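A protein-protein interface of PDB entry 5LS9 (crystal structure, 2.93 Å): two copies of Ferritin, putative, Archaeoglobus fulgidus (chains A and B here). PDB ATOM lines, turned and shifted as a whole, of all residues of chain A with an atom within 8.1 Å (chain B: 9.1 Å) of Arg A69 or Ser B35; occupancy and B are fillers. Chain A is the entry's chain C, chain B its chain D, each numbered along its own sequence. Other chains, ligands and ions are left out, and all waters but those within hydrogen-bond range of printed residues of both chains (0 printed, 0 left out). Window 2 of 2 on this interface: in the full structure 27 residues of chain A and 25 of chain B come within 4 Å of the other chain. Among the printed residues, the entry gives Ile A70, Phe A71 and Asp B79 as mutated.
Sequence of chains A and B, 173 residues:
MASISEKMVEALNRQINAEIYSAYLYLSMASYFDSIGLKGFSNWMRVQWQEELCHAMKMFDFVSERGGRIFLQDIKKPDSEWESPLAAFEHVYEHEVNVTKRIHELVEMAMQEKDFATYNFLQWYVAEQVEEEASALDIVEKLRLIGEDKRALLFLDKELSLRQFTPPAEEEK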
ATOM      1  N   ILE A   4      27.997  32.145  -5.388  1.00  0.00           N
ATOM      2  CA  ILE A   4      26.605  32.620  -5.382  1.00  0.00           C
ATOM      3  C   ILE A   4      26.342  33.822  -4.451  1.00  0.00           C
ATOM      4  O   ILE A   4      26.385  33.700  -3.226  1.00  0.00           O
ATOM      5  CB  ILE A   4      25.610  31.468  -5.079  1.00  0.00           C
ATOM      6  CG1 ILE A   4      24.166  31.955  -5.246  1.00  0.00           C
ATOM      7  CG2 ILE A   4      25.824  30.886  -3.689  1.00  0.00           C
ATOM      8  CD1 ILE A   4      23.114  30.856  -5.249  1.00  0.00           C
ATOM      9  N   GLU A   6      24.425  36.766  -2.382  1.00  0.00           N
ATOM     10  CA  GLU A   6      23.233  36.719  -1.543  1.00  0.00           C
ATOM     11  C   GLU A   6      21.970  37.152  -2.297  1.00  0.00           C
ATOM     12  O   GLU A   6      20.896  36.590  -2.095  1.00  0.00           O
ATOM     13  CB  GLU A   6      23.435  37.576  -0.293  1.00  0.00           C
ATOM     14  CG  GLU A   6      24.463  36.986   0.656  1.00  0.00           C
ATOM     15  CD  GLU A   6      24.041  35.622   1.160  1.00  0.00           C
ATOM     16  OE1 GLU A   6      23.097  35.566   1.978  1.00  0.00           O
ATOM     17  OE2 GLU A   6      24.637  34.611   0.724  1.00  0.00           O
ATOM     18  N   MET A   8      20.947  36.551  -5.292  1.00  0.00           N
ATOM     19  CA  MET A   8      20.310  35.377  -5.908  1.00  0.00           C
ATOM     20  C   MET A   8      19.670  34.468  -4.857  1.00  0.00           C
ATOM     21  O   MET A   8      18.499  34.110  -4.979  1.00  0.00           O
ATOM     22  CB  MET A   8      21.300  34.558  -6.756  1.00  0.00           C
ATOM     23  CG  MET A   8      21.617  35.141  -8.124  1.00  0.00           C
ATOM     24  SD  MET A   8      20.209  35.757  -9.081  1.00  0.00           S
ATOM     25  CE  MET A   8      19.651  34.268  -9.894  1.00  0.00           C
ATOM     26  N   VAL A   9      20.426  34.104  -3.825  1.00  0.00           N
ATOM     27  CA  VAL A   9      19.917  33.191  -2.805  1.00  0.00           C
ATOM     28  C   VAL A   9      18.600  33.684  -2.205  1.00  0.00           C
ATOM     29  O   VAL A   9      17.741  32.879  -1.861  1.00  0.00           O
ATOM     30  CB  VAL A   9      20.957  32.948  -1.694  1.00  0.00           C
ATOM     31  CG1 VAL A   9      20.322  32.262  -0.493  1.00  0.00           C
ATOM     32  CG2 VAL A   9      22.099  32.097  -2.223  1.00  0.00           C
ATOM     33  N   GLU A  10      18.457  35.003  -2.070  1.00  0.00           N
ATOM     34  CA  GLU A  10      17.185  35.627  -1.664  1.00  0.00           C
ATOM     35  C   GLU A  10      16.108  35.435  -2.735  1.00  0.00           C
ATOM     36  O   GLU A  10      15.022  34.914  -2.459  1.00  0.00           O
ATOM     37  CB  GLU A  10      17.386  37.135  -1.403  1.00  0.00           C
ATOM     38  CG  GLU A  10      16.109  37.985  -1.298  1.00  0.00           C
ATOM     39  CD  GLU A  10      15.662  38.291   0.124  1.00  0.00           C
ATOM     40  OE1 GLU A  10      16.068  37.579   1.066  1.00  0.00           O
ATOM     41  OE2 GLU A  10      14.886  39.259   0.296  1.00  0.00           O
ATOM     42  N   LEU A  12      15.836  33.497  -5.220  1.00  0.00           N
ATOM     43  CA  LEU A  12      15.488  32.094  -5.454  1.00  0.00           C
ATOM     44  C   LEU A  12      14.568  31.538  -4.363  1.00  0.00           C
ATOM     45  O   LEU A  12      13.567  30.880  -4.669  1.00  0.00           O
ATOM     46  CB  LEU A  12      16.755  31.237  -5.564  1.00  0.00           C
ATOM     47  CG  LEU A  12      17.605  31.445  -6.816  1.00  0.00           C
ATOM     48  CD1 LEU A  12      18.979  30.821  -6.644  1.00  0.00           C
ATOM     49  CD2 LEU A  12      16.908  30.848  -8.022  1.00  0.00           C
ATOM     50  N   ASN A  13      14.905  31.810  -3.101  1.00  0.00           N
ATOM     51  CA  ASN A  13      14.041  31.427  -1.984  1.00  0.00           C
ATOM     52  C   ASN A  13      12.610  31.978  -2.151  1.00  0.00           C
ATOM     53  O   ASN A  13      11.633  31.325  -1.752  1.00  0.00           O
ATOM     54  CB  ASN A  13      14.644  31.887  -0.651  1.00  0.00           C
ATOM     55  CG  ASN A  13      15.929  31.154  -0.301  1.00  0.00           C
ATOM     56  OD1 ASN A  13      16.319  30.205  -0.978  1.00  0.00           O
ATOM     57  ND2 ASN A  13      16.602  31.603   0.759  1.00  0.00           N
ATOM     58  N   ILE A  16      11.029  29.634  -4.899  1.00  0.00           N
ATOM     59  CA  ILE A  16      10.671  28.404  -4.192  1.00  0.00           C
ATOM     60  C   ILE A  16       9.330  28.614  -3.477  1.00  0.00           C
ATOM     61  O   ILE A  16       8.376  27.857  -3.676  1.00  0.00           O
ATOM     62  CB  ILE A  16      11.793  27.994  -3.182  1.00  0.00           C
ATOM     63  CG1 ILE A  16      13.058  27.537  -3.936  1.00  0.00           C
ATOM     64  CG2 ILE A  16      11.332  26.859  -2.257  1.00  0.00           C
ATOM     65  CD1 ILE A  16      14.326  27.472  -3.103  1.00  0.00           C
ATOM     66  N   PHE A  60      15.425  23.835  -4.712  1.00  0.00           N
ATOM     67  CA  PHE A  60      15.927  23.532  -3.369  1.00  0.00           C
ATOM     68  C   PHE A  60      17.302  22.886  -3.464  1.00  0.00           C
ATOM     69  O   PHE A  60      18.251  23.370  -2.852  1.00  0.00           O
ATOM     70  CB  PHE A  60      14.942  22.597  -2.647  1.00  0.00           C
ATOM     71  CG  PHE A  60      15.231  22.379  -1.179  1.00  0.00           C
ATOM     72  CD1 PHE A  60      16.308  21.594  -0.764  1.00  0.00           C
ATOM     73  CD2 PHE A  60      14.384  22.903  -0.207  1.00  0.00           C
ATOM     74  CE1 PHE A  60      16.549  21.376   0.586  1.00  0.00           C
ATOM     75  CE2 PHE A  60      14.617  22.676   1.141  1.00  0.00           C
ATOM     76  CZ  PHE A  60      15.698  21.915   1.539  1.00  0.00           C
ATOM     77  N   VAL A  63      20.134  25.284  -5.013  1.00  0.00           N
ATOM     78  CA  VAL A  63      20.592  26.295  -4.051  1.00  0.00           C
ATOM     79  C   VAL A  63      21.471  25.632  -2.994  1.00  0.00           C
ATOM     80  O   VAL A  63      22.610  26.050  -2.754  1.00  0.00           O
ATOM     81  CB  VAL A  63      19.412  27.015  -3.368  1.00  0.00           C
ATOM     82  CG1 VAL A  63      19.891  27.847  -2.189  1.00  0.00           C
ATOM     83  CG2 VAL A  63      18.691  27.918  -4.354  1.00  0.00           C
ATOM     84  N   SER A  64      20.941  24.577  -2.388  1.00  0.00           N
ATOM     85  CA  SER A  64      21.671  23.820  -1.382  1.00  0.00           C
ATOM     86  C   SER A  64      22.986  23.264  -1.943  1.00  0.00           C
ATOM     87  O   SER A  64      24.026  23.361  -1.299  1.00  0.00           O
ATOM     88  CB  SER A  64      20.787  22.694  -0.842  1.00  0.00           C
ATOM     89  OG  SER A  64      21.433  21.992   0.191  1.00  0.00           O
ATOM     90  N   ARG A  66      24.734  24.558  -4.107  1.00  0.00           N
ATOM     91  CA  ARG A  66      25.584  25.726  -4.405  1.00  0.00           C
ATOM     92  C   ARG A  66      25.985  26.614  -3.194  1.00  0.00           C
ATOM     93  O   ARG A  66      26.559  27.706  -3.373  1.00  0.00           O
ATOM     94  CB  ARG A  66      24.858  26.597  -5.432  1.00  0.00           C
ATOM     95  CG  ARG A  66      24.957  26.099  -6.867  1.00  0.00           C
ATOM     96  CD  ARG A  66      25.919  26.948  -7.687  1.00  0.00           C
ATOM     97  NE  ARG A  66      25.339  28.249  -8.031  1.00  0.00           N
ATOM     98  CZ  ARG A  66      26.050  29.329  -8.342  1.00  0.00           C
ATOM     99  NH1 ARG A  66      27.372  29.298  -8.329  1.00  0.00           N
ATOM    100  NH2 ARG A  66      25.448  30.463  -8.649  1.00  0.00           N
ATOM    101  N   GLY A  67      25.663  26.168  -1.979  1.00  0.00           N
ATOM    102  CA  GLY A  67      26.115  26.840  -0.746  1.00  0.00           C
ATOM    103  C   GLY A  67      25.128  27.796  -0.083  1.00  0.00           C
ATOM    104  O   GLY A  67      25.320  28.199   1.071  1.00  0.00           O
ATOM    105  N   GLY A  68      24.072  28.166  -0.797  1.00  0.00           N
ATOM    106  CA  GLY A  68      23.093  29.123  -0.281  1.00  0.00           C
ATOM    107  C   GLY A  68      22.249  28.520   0.819  1.00  0.00           C
ATOM    108  O   GLY A  68      22.123  27.306   0.913  1.00  0.00           O
ATOM    109  N   ARG A  69      21.668  29.376   1.653  1.00  0.00           N
ATOM    110  CA  ARG A  69      20.839  28.929   2.761  1.00  0.00           C
ATOM    111  C   ARG A  69      19.352  29.132   2.440  1.00  0.00           C
ATOM    112  O   ARG A  69      18.909  30.234   2.083  1.00  0.00           O
ATOM    113  CB  ARG A  69      21.238  29.670   4.035  1.00  0.00           C
ATOM    114  CG  ARG A  69      20.344  29.401   5.233  1.00  0.00           C
ATOM    115  CD  ARG A  69      20.605  28.043   5.871  1.00  0.00           C
ATOM    116  NE  ARG A  69      19.423  27.572   6.596  1.00  0.00           N
ATOM    117  CZ  ARG A  69      19.432  26.796   7.676  1.00  0.00           C
ATOM    118  NH1 ARG A  69      20.565  26.388   8.213  1.00  0.00           N
ATOM    119  NH2 ARG A  69      18.281  26.436   8.234  1.00  0.00           N
ATOM    120  N   ILE A  70      18.586  28.058   2.590  1.00  0.00           N
ATOM    121  CA  ILE A  70      17.184  28.041   2.199  1.00  0.00           C
ATOM    122  C   ILE A  70      16.333  28.207   3.449  1.00  0.00           C
ATOM    123  O   ILE A  70      16.439  27.395   4.368  1.00  0.00           O
ATOM    124  CB  ILE A  70      16.808  26.707   1.496  1.00  0.00           C
ATOM    125  CG1 ILE A  70      17.713  26.446   0.291  1.00  0.00           C
ATOM    126  CG2 ILE A  70      15.372  26.735   1.018  1.00  0.00           C
ATOM    127  CD1 ILE A  70      18.831  25.470   0.561  1.00  0.00           C
ATOM    128  N   PHE A  71      15.499  29.249   3.476  1.00  0.00           N
ATOM    129  CA  PHE A  71      14.540  29.451   4.547  1.00  0.00           C
ATOM    130  C   PHE A  71      13.144  29.372   3.993  1.00  0.00           C
ATOM    131  O   PHE A  71      12.851  29.988   2.964  1.00  0.00           O
ATOM    132  CB  PHE A  71      14.701  30.834   5.172  1.00  0.00           C
ATOM    133  CG  PHE A  71      15.955  31.001   5.971  1.00  0.00           C
ATOM    134  CD1 PHE A  71      16.216  30.186   7.046  1.00  0.00           C
ATOM    135  CD2 PHE A  71      16.858  32.004   5.659  1.00  0.00           C
ATOM    136  CE1 PHE A  71      17.368  30.344   7.787  1.00  0.00           C
ATOM    137  CE2 PHE A  71      18.014  32.173   6.398  1.00  0.00           C
ATOM    138  CZ  PHE A  71      18.271  31.345   7.469  1.00  0.00           C
ATOM    139  N   LEU A  72      12.271  28.659   4.704  1.00  0.00           N
ATOM    140  CA  LEU A  72      10.880  28.493   4.276  1.00  0.00           C
ATOM    141  C   LEU A  72       9.947  29.488   4.943  1.00  0.00           C
ATOM    142  O   LEU A  72       9.756  29.442   6.150  1.00  0.00           O
ATOM    143  CB  LEU A  72      10.417  27.086   4.587  1.00  0.00           C
ATOM    144  CG  LEU A  72      11.105  25.998   3.776  1.00  0.00           C
ATOM    145  CD1 LEU A  72      10.744  24.628   4.337  1.00  0.00           C
ATOM    146  CD2 LEU A  72      10.754  26.078   2.294  1.00  0.00           C
ATOM    147  N   LEU B  27      10.565  19.718   6.205  1.00  0.00           N
ATOM    148  CA  LEU B  27      11.252  20.269   5.051  1.00  0.00           C
ATOM    149  C   LEU B  27      12.337  21.262   5.472  1.00  0.00           C
ATOM    150  O   LEU B  27      13.442  21.199   4.956  1.00  0.00           O
ATOM    151  CB  LEU B  27      10.272  20.914   4.060  1.00  0.00           C
ATOM    152  CG  LEU B  27      10.903  21.410   2.752  1.00  0.00           C
ATOM    153  CD1 LEU B  27      11.485  20.235   1.981  1.00  0.00           C
ATOM    154  CD2 LEU B  27       9.923  22.192   1.877  1.00  0.00           C
ATOM    155  N   SER B  28      12.045  22.165   6.408  1.00  0.00           N
ATOM    156  CA  SER B  28      13.045  23.165   6.788  1.00  0.00           C
ATOM    157  C   SER B  28      14.265  22.526   7.482  1.00  0.00           C
ATOM    158  O   SER B  28      15.408  22.973   7.282  1.00  0.00           O
ATOM    159  CB  SER B  28      12.443  24.261   7.666  1.00  0.00           C
ATOM    160  OG  SER B  28      13.253  25.430   7.594  1.00  0.00           O
ATOM    161  N   MET B  29      14.027  21.494   8.292  1.00  0.00           N
ATOM    162  CA  MET B  29      15.121  20.793   8.950  1.00  0.00           C
ATOM    163  C   MET B  29      16.082  20.292   7.899  1.00  0.00           C
ATOM    164  O   MET B  29      17.298  20.301   8.113  1.00  0.00           O
ATOM    165  CB  MET B  29      14.629  19.617   9.781  1.00  0.00           C
ATOM    166  CG  MET B  29      13.955  20.034  11.062  1.00  0.00           C
ATOM    167  SD  MET B  29      13.546  18.646  12.145  1.00  0.00           S
ATOM    168  CE  MET B  29      12.355  19.470  13.198  1.00  0.00           C
ATOM    169  N   ALA B  30      15.551  19.854   6.762  1.00  0.00           N
ATOM    170  CA  ALA B  30      16.404  19.431   5.661  1.00  0.00           C
ATOM    171  C   ALA B  30      17.384  20.534   5.269  1.00  0.00           C
ATOM    172  O   ALA B  30      18.595  20.308   5.260  1.00  0.00           O
ATOM    173  CB  ALA B  30      15.575  19.012   4.468  1.00  0.00           C
ATOM    174  N   SER B  31      16.867  21.727   4.974  1.00  0.00           N
ATOM    175  CA  SER B  31      17.728  22.875   4.678  1.00  0.00           C
ATOM    176  C   SER B  31      18.726  23.124   5.796  1.00  0.00           C
ATOM    177  O   SER B  31      19.892  23.434   5.519  1.00  0.00           O
ATOM    178  CB  SER B  31      16.919  24.144   4.454  1.00  0.00           C
ATOM    179  OG  SER B  31      17.783  25.212   4.102  1.00  0.00           O
ATOM    180  N   TYR B  32      18.265  22.999   7.048  1.00  0.00           N
ATOM    181  CA  TYR B  32      19.138  23.148   8.225  1.00  0.00           C
ATOM    182  C   TYR B  32      20.295  22.175   8.130  1.00  0.00           C
ATOM    183  O   TYR B  32      21.463  22.584   8.130  1.00  0.00           O
ATOM    184  CB  TYR B  32      18.360  22.949   9.548  1.00  0.00           C
ATOM    185  CG  TYR B  32      19.218  22.654  10.775  1.00  0.00           C
ATOM    186  CD1 TYR B  32      20.237  23.524  11.167  1.00  0.00           C
ATOM    187  CD2 TYR B  32      19.002  21.510  11.552  1.00  0.00           C
ATOM    188  CE1 TYR B  32      21.019  23.260  12.283  1.00  0.00           C
ATOM    189  CE2 TYR B  32      19.778  21.243  12.671  1.00  0.00           C
ATOM    190  CZ  TYR B  32      20.785  22.120  13.031  1.00  0.00           C
ATOM    191  OH  TYR B  32      21.571  21.863  14.129  1.00  0.00           O
ATOM    192  N   PHE B  33      19.964  20.890   8.011  1.00  0.00           N
ATOM    193  CA  PHE B  33      20.984  19.838   7.990  1.00  0.00           C
ATOM    194  C   PHE B  33      21.933  19.943   6.796  1.00  0.00           C
ATOM    195  O   PHE B  33      23.029  19.399   6.838  1.00  0.00           O
ATOM    196  CB  PHE B  33      20.334  18.450   8.030  1.00  0.00           C
ATOM    197  CG  PHE B  33      19.901  18.008   9.414  1.00  0.00           C
ATOM    198  CD1 PHE B  33      20.850  17.756  10.416  1.00  0.00           C
ATOM    199  CD2 PHE B  33      18.551  17.799   9.706  1.00  0.00           C
ATOM    200  CE1 PHE B  33      20.455  17.325  11.674  1.00  0.00           C
ATOM    201  CE2 PHE B  33      18.158  17.370  10.970  1.00  0.00           C
ATOM    202  CZ  PHE B  33      19.112  17.132  11.952  1.00  0.00           C
ATOM    203  N   ASP B  34      21.511  20.626   5.733  1.00  0.00           N
ATOM    204  CA  ASP B  34      22.371  20.843   4.551  1.00  0.00           C
ATOM    205  C   ASP B  34      23.436  21.896   4.834  1.00  0.00           C
ATOM    206  O   ASP B  34      24.590  21.750   4.420  1.00  0.00           O
ATOM    207  CB  ASP B  34      21.546  21.284   3.321  1.00  0.00           C
ATOM    208  CG  ASP B  34      20.696  20.151   2.705  1.00  0.00           C
ATOM    209  OD1 ASP B  34      21.051  18.947   2.789  1.00  0.00           O
ATOM    210  OD2 ASP B  34      19.654  20.497   2.104  1.00  0.00           O
ATOM    211  N   SER B  35      23.031  22.955   5.538  1.00  0.00           N
ATOM    212  CA  SER B  35      23.927  24.058   5.903  1.00  0.00           C
ATOM    213  C   SER B  35      25.035  23.619   6.872  1.00  0.00           C
ATOM    214  O   SER B  35      26.185  24.046   6.741  1.00  0.00           O
ATOM    215  CB  SER B  35      23.119  25.201   6.510  1.00  0.00           C
ATOM    216  OG  SER B  35      22.343  24.721   7.579  1.00  0.00           O
ATOM    217  N   ILE B  36      24.689  22.767   7.837  1.00  0.00           N
ATOM    218  CA  ILE B  36      25.706  22.141   8.686  1.00  0.00           C
ATOM    219  C   ILE B  36      26.173  20.788   8.145  1.00  0.00           C
ATOM    220  O   ILE B  36      26.663  19.958   8.908  1.00  0.00           O
ATOM    221  CB  ILE B  36      25.242  21.973  10.145  1.00  0.00           C
ATOM    222  CG1 ILE B  36      23.999  21.083  10.232  1.00  0.00           C
ATOM    223  CG2 ILE B  36      24.976  23.327  10.771  1.00  0.00           C
ATOM    224  CD1 ILE B  36      23.777  20.503  11.613  1.00  0.00           C
ATOM    225  N   GLY B  37      25.982  20.554   6.849  1.00  0.00           N
ATOM    226  CA  GLY B  37      26.726  19.533   6.107  1.00  0.00           C
ATOM    227  C   GLY B  37      26.412  18.075   6.358  1.00  0.00           C
ATOM    228  O   GLY B  37      27.265  17.231   6.114  1.00  0.00           O
ATOM    229  N   LEU B  38      25.193  17.775   6.811  1.00  0.00           N
ATOM    230  CA  LEU B  38      24.779  16.394   7.127  1.00  0.00           C
ATOM    231  C   LEU B  38      23.702  15.881   6.155  1.00  0.00           C
ATOM    232  O   LEU B  38      22.490  16.062   6.370  1.00  0.00           O
ATOM    233  CB  LEU B  38      24.297  16.303   8.579  1.00  0.00           C
ATOM    234  CG  LEU B  38      25.335  16.612   9.677  1.00  0.00           C
ATOM    235  CD1 LEU B  38      24.689  16.658  11.065  1.00  0.00           C
ATOM    236  CD2 LEU B  38      26.494  15.616   9.653  1.00  0.00           C
ATOM    237  N   LYS B  39      24.163  15.213   5.096  1.00  0.00           N
ATOM    238  CA  LYS B  39      23.311  14.896   3.946  1.00  0.00           C
ATOM    239  C   LYS B  39      22.243  13.854   4.297  1.00  0.00           C
ATOM    240  O   LYS B  39      21.107  13.927   3.813  1.00  0.00           O
ATOM    241  CB  LYS B  39      24.157  14.403   2.754  1.00  0.00           C
ATOM    242  CG  LYS B  39      25.336  15.286   2.340  1.00  0.00           C
ATOM    243  CD  LYS B  39      24.945  16.467   1.455  1.00  0.00           C
ATOM    244  CE  LYS B  39      24.245  17.577   2.225  1.00  0.00           C
ATOM    245  NZ  LYS B  39      24.278  18.880   1.508  1.00  0.00           N
ATOM    246  N   SER B  42      19.541  15.223   6.417  1.00  0.00           N
ATOM    247  CA  SER B  42      18.651  15.917   5.474  1.00  0.00           C
ATOM    248  C   SER B  42      17.747  14.965   4.700  1.00  0.00           C
ATOM    249  O   SER B  42      16.547  15.218   4.579  1.00  0.00           O
ATOM    250  CB  SER B  42      19.445  16.747   4.475  1.00  0.00           C
ATOM    251  OG  SER B  42      18.561  17.464   3.631  1.00  0.00           O
ATOM    252  N   PRO B  78       7.911  27.743   9.668  1.00  0.00           N
ATOM    253  CA  PRO B  78       8.549  26.818  10.624  1.00  0.00           C
ATOM    254  C   PRO B  78       9.883  27.291  11.207  1.00  0.00           C
ATOM    255  O   PRO B  78      10.575  28.107  10.611  1.00  0.00           O
ATOM    256  CB  PRO B  78       8.790  25.558   9.785  1.00  0.00           C
ATOM    257  CG  PRO B  78       8.959  26.065   8.401  1.00  0.00           C
ATOM    258  CD  PRO B  78       8.059  27.269   8.281  1.00  0.00           C
ATOM    259  N   ASP B  79      10.239  26.753  12.369  1.00  0.00           N
ATOM    260  CA  ASP B  79      11.499  27.105  13.017  1.00  0.00           C
ATOM    261  C   ASP B  79      12.600  26.694  12.045  1.00  0.00           C
ATOM    262  O   ASP B  79      12.562  25.585  11.525  1.00  0.00           O
ATOM    263  CB  ASP B  79      11.684  26.355  14.351  1.00  0.00           C
ATOM    264  CG  ASP B  79      10.518  26.556  15.350  1.00  0.00           C
ATOM    265  OD1 ASP B  79       9.683  27.476  15.184  1.00  0.00           O
ATOM    266  OD2 ASP B  79      10.449  25.768  16.318  1.00  0.00           O
ATOM    267  N   SER B  80      13.560  27.576  11.771  1.00  0.00           N
ATOM    268  CA  SER B  80      14.598  27.282  10.776  1.00  0.00           C
ATOM    269  C   SER B  80      15.965  26.925  11.368  1.00  0.00           C
ATOM    270  O   SER B  80      16.857  26.493  10.635  1.00  0.00           O
ATOM    271  CB  SER B  80      14.746  28.458   9.812  1.00  0.00           C
ATOM    272  OG  SER B  80      15.607  29.453  10.323  1.00  0.00           O
ATOM    273  N   GLU B  81      16.138  27.109  12.678  1.00  0.00           N
ATOM    274  CA  GLU B  81      17.443  26.881  13.323  1.00  0.00           C
ATOM    275  C   GLU B  81      17.342  26.034  14.597  1.00  0.00           C
ATOM    276  O   GLU B  81      16.351  26.080  15.320  1.00  0.00           O
ATOM    277  CB  GLU B  81      18.131  28.220  13.641  1.00  0.00           C
ATOM    278  CG  GLU B  81      18.858  28.880  12.464  1.00  0.00           C
ATOM    279  CD  GLU B  81      20.215  28.254  12.137  1.00  0.00           C
ATOM    280  OE1 GLU B  81      20.449  27.077  12.484  1.00  0.00           O
ATOM    281  OE2 GLU B  81      21.057  28.941  11.517  1.00  0.00           O
ATOM    282  N   TRP B  82      18.379  25.248  14.853  1.00  0.00           N
ATOM    283  CA  TRP B  82      18.473  24.458  16.070  1.00  0.00           C
ATOM    284  C   TRP B  82      19.934  24.388  16.491  1.00  0.00           C
ATOM    285  O   TRP B  82      20.831  24.439  15.647  1.00  0.00           O
ATOM    286  CB  TRP B  82      17.930  23.050  15.849  1.00  0.00           C
ATOM    287  CG  TRP B  82      16.439  22.975  15.689  1.00  0.00           C
ATOM    288  CD1 TRP B  82      15.509  22.757  16.673  1.00  0.00           C
ATOM    289  CD2 TRP B  82      15.706  23.102  14.470  1.00  0.00           C
ATOM    290  NE1 TRP B  82      14.237  22.748  16.138  1.00  0.00           N
ATOM    291  CE2 TRP B  82      14.332  22.955  14.788  1.00  0.00           C
ATOM    292  CE3 TRP B  82      16.073  23.327  13.140  1.00  0.00           C
ATOM    293  CZ2 TRP B  82      13.333  23.025  13.823  1.00  0.00           C
ATOM    294  CZ3 TRP B  82      15.078  23.401  12.183  1.00  0.00           C
ATOM    295  CH2 TRP B  82      13.722  23.246  12.530  1.00  0.00           C
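The side-chain amide nitrogen (ND2) of Asn A13 sits at hydrogen-bond distance from the backbone carbonyl oxygen (O) of Arg A69 (3.0 Å).
The backbone carbonyl oxygen (O) of Trp B82 is in hydrogen-bond range of the side-chain hydroxyl (OH) of Tyr B32, 3.1 Å away.
The side-chain hydroxyl (OG) of Ser B42 is in hydrogen-bond range of the side-chain carboxylate (OD1) of Asp B34, at 3.0 Å.
The side-chain carboxylate of Asp B34 is in salt-bridge range of the side-chain amino group of Lys B39.
The backbone carbonyl oxygen of Ser B31 is in hydrogen-bond range of the side-chain hydroxyl of Ser B35 (3.5 Å).
Of the 19 printed residues of chain B, 8 touch a printed residue of chain A.
Hydrophobic or aromatic side chains of chain B that line the printed part of chain A: Leu B27, Tyr B32 and Pro B78.
Among the printed residues, 12 pairs touch across the chains.
Among the printed residues, no Asp or Glu carboxylate lies within 4 Å of a Lys or Arg side-chain nitrogen of the other chain.
Printed residues of chain B within 4 Å of Ser A64: Asp B34.
Of chain B, only Ser B31, Tyr B32, Ser B35 and Ser B80 come within 4 Å of Arg A69.
Of the printed residues of chain B, Phe A71 touches Ser B80 (3.2 Å).
Printed residues of chain A within 4 Å of Tyr B32: Arg A69 (3.4 Å).
Of chain A, only Arg A69 (2.5 Å) comes within 4 Å of Ser B35.
Printed residues of chain A within 4 Å of Pro B78: Leu A72.
Of the printed residues of chain A, Ser B80 touches Arg A69 and Phe A71.
The nearest residue of chain B that does not touch Arg A69 is Glu B81 (4.2 Å).
The nearest printed residue of chain A that does not touch Pro B78 is Phe A71 (6.9 Å).
OG of Ser A64 is in hydrogen-bond range of OD2 of Asp B34.
The guanidinium group (NH2) of Arg A69 sits at hydrogen-bond distance from the backbone carbonyl oxygen (O) of Ser B80, 2.8 Å away.
O of Ile A70 is in hydrogen-bond range of OG of Ser B31, at 2.6 Å.
The side-chain hydroxyl of Ser B35 is in hydrogen-bond range of the guanidinium group of Arg A69, at 2.5 Å.
Among the printed residues, merely in contact across the chains: Phe A60 with Ser B31 (3.6 Å), Phe A60 with Asp B34 (3.6 Å), Arg A69 with Ser B31 (3.8 Å), Arg A69 with Tyr B32 (3.4 Å), Phe A71 with Ser B80 (3.2 Å), Leu A72 with Leu B27 (3.6 Å), Leu A72 with Ser B28 (3.5 Å) and Leu A72 with Pro B78 (3.5 Å).
No position is printed for both chains.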
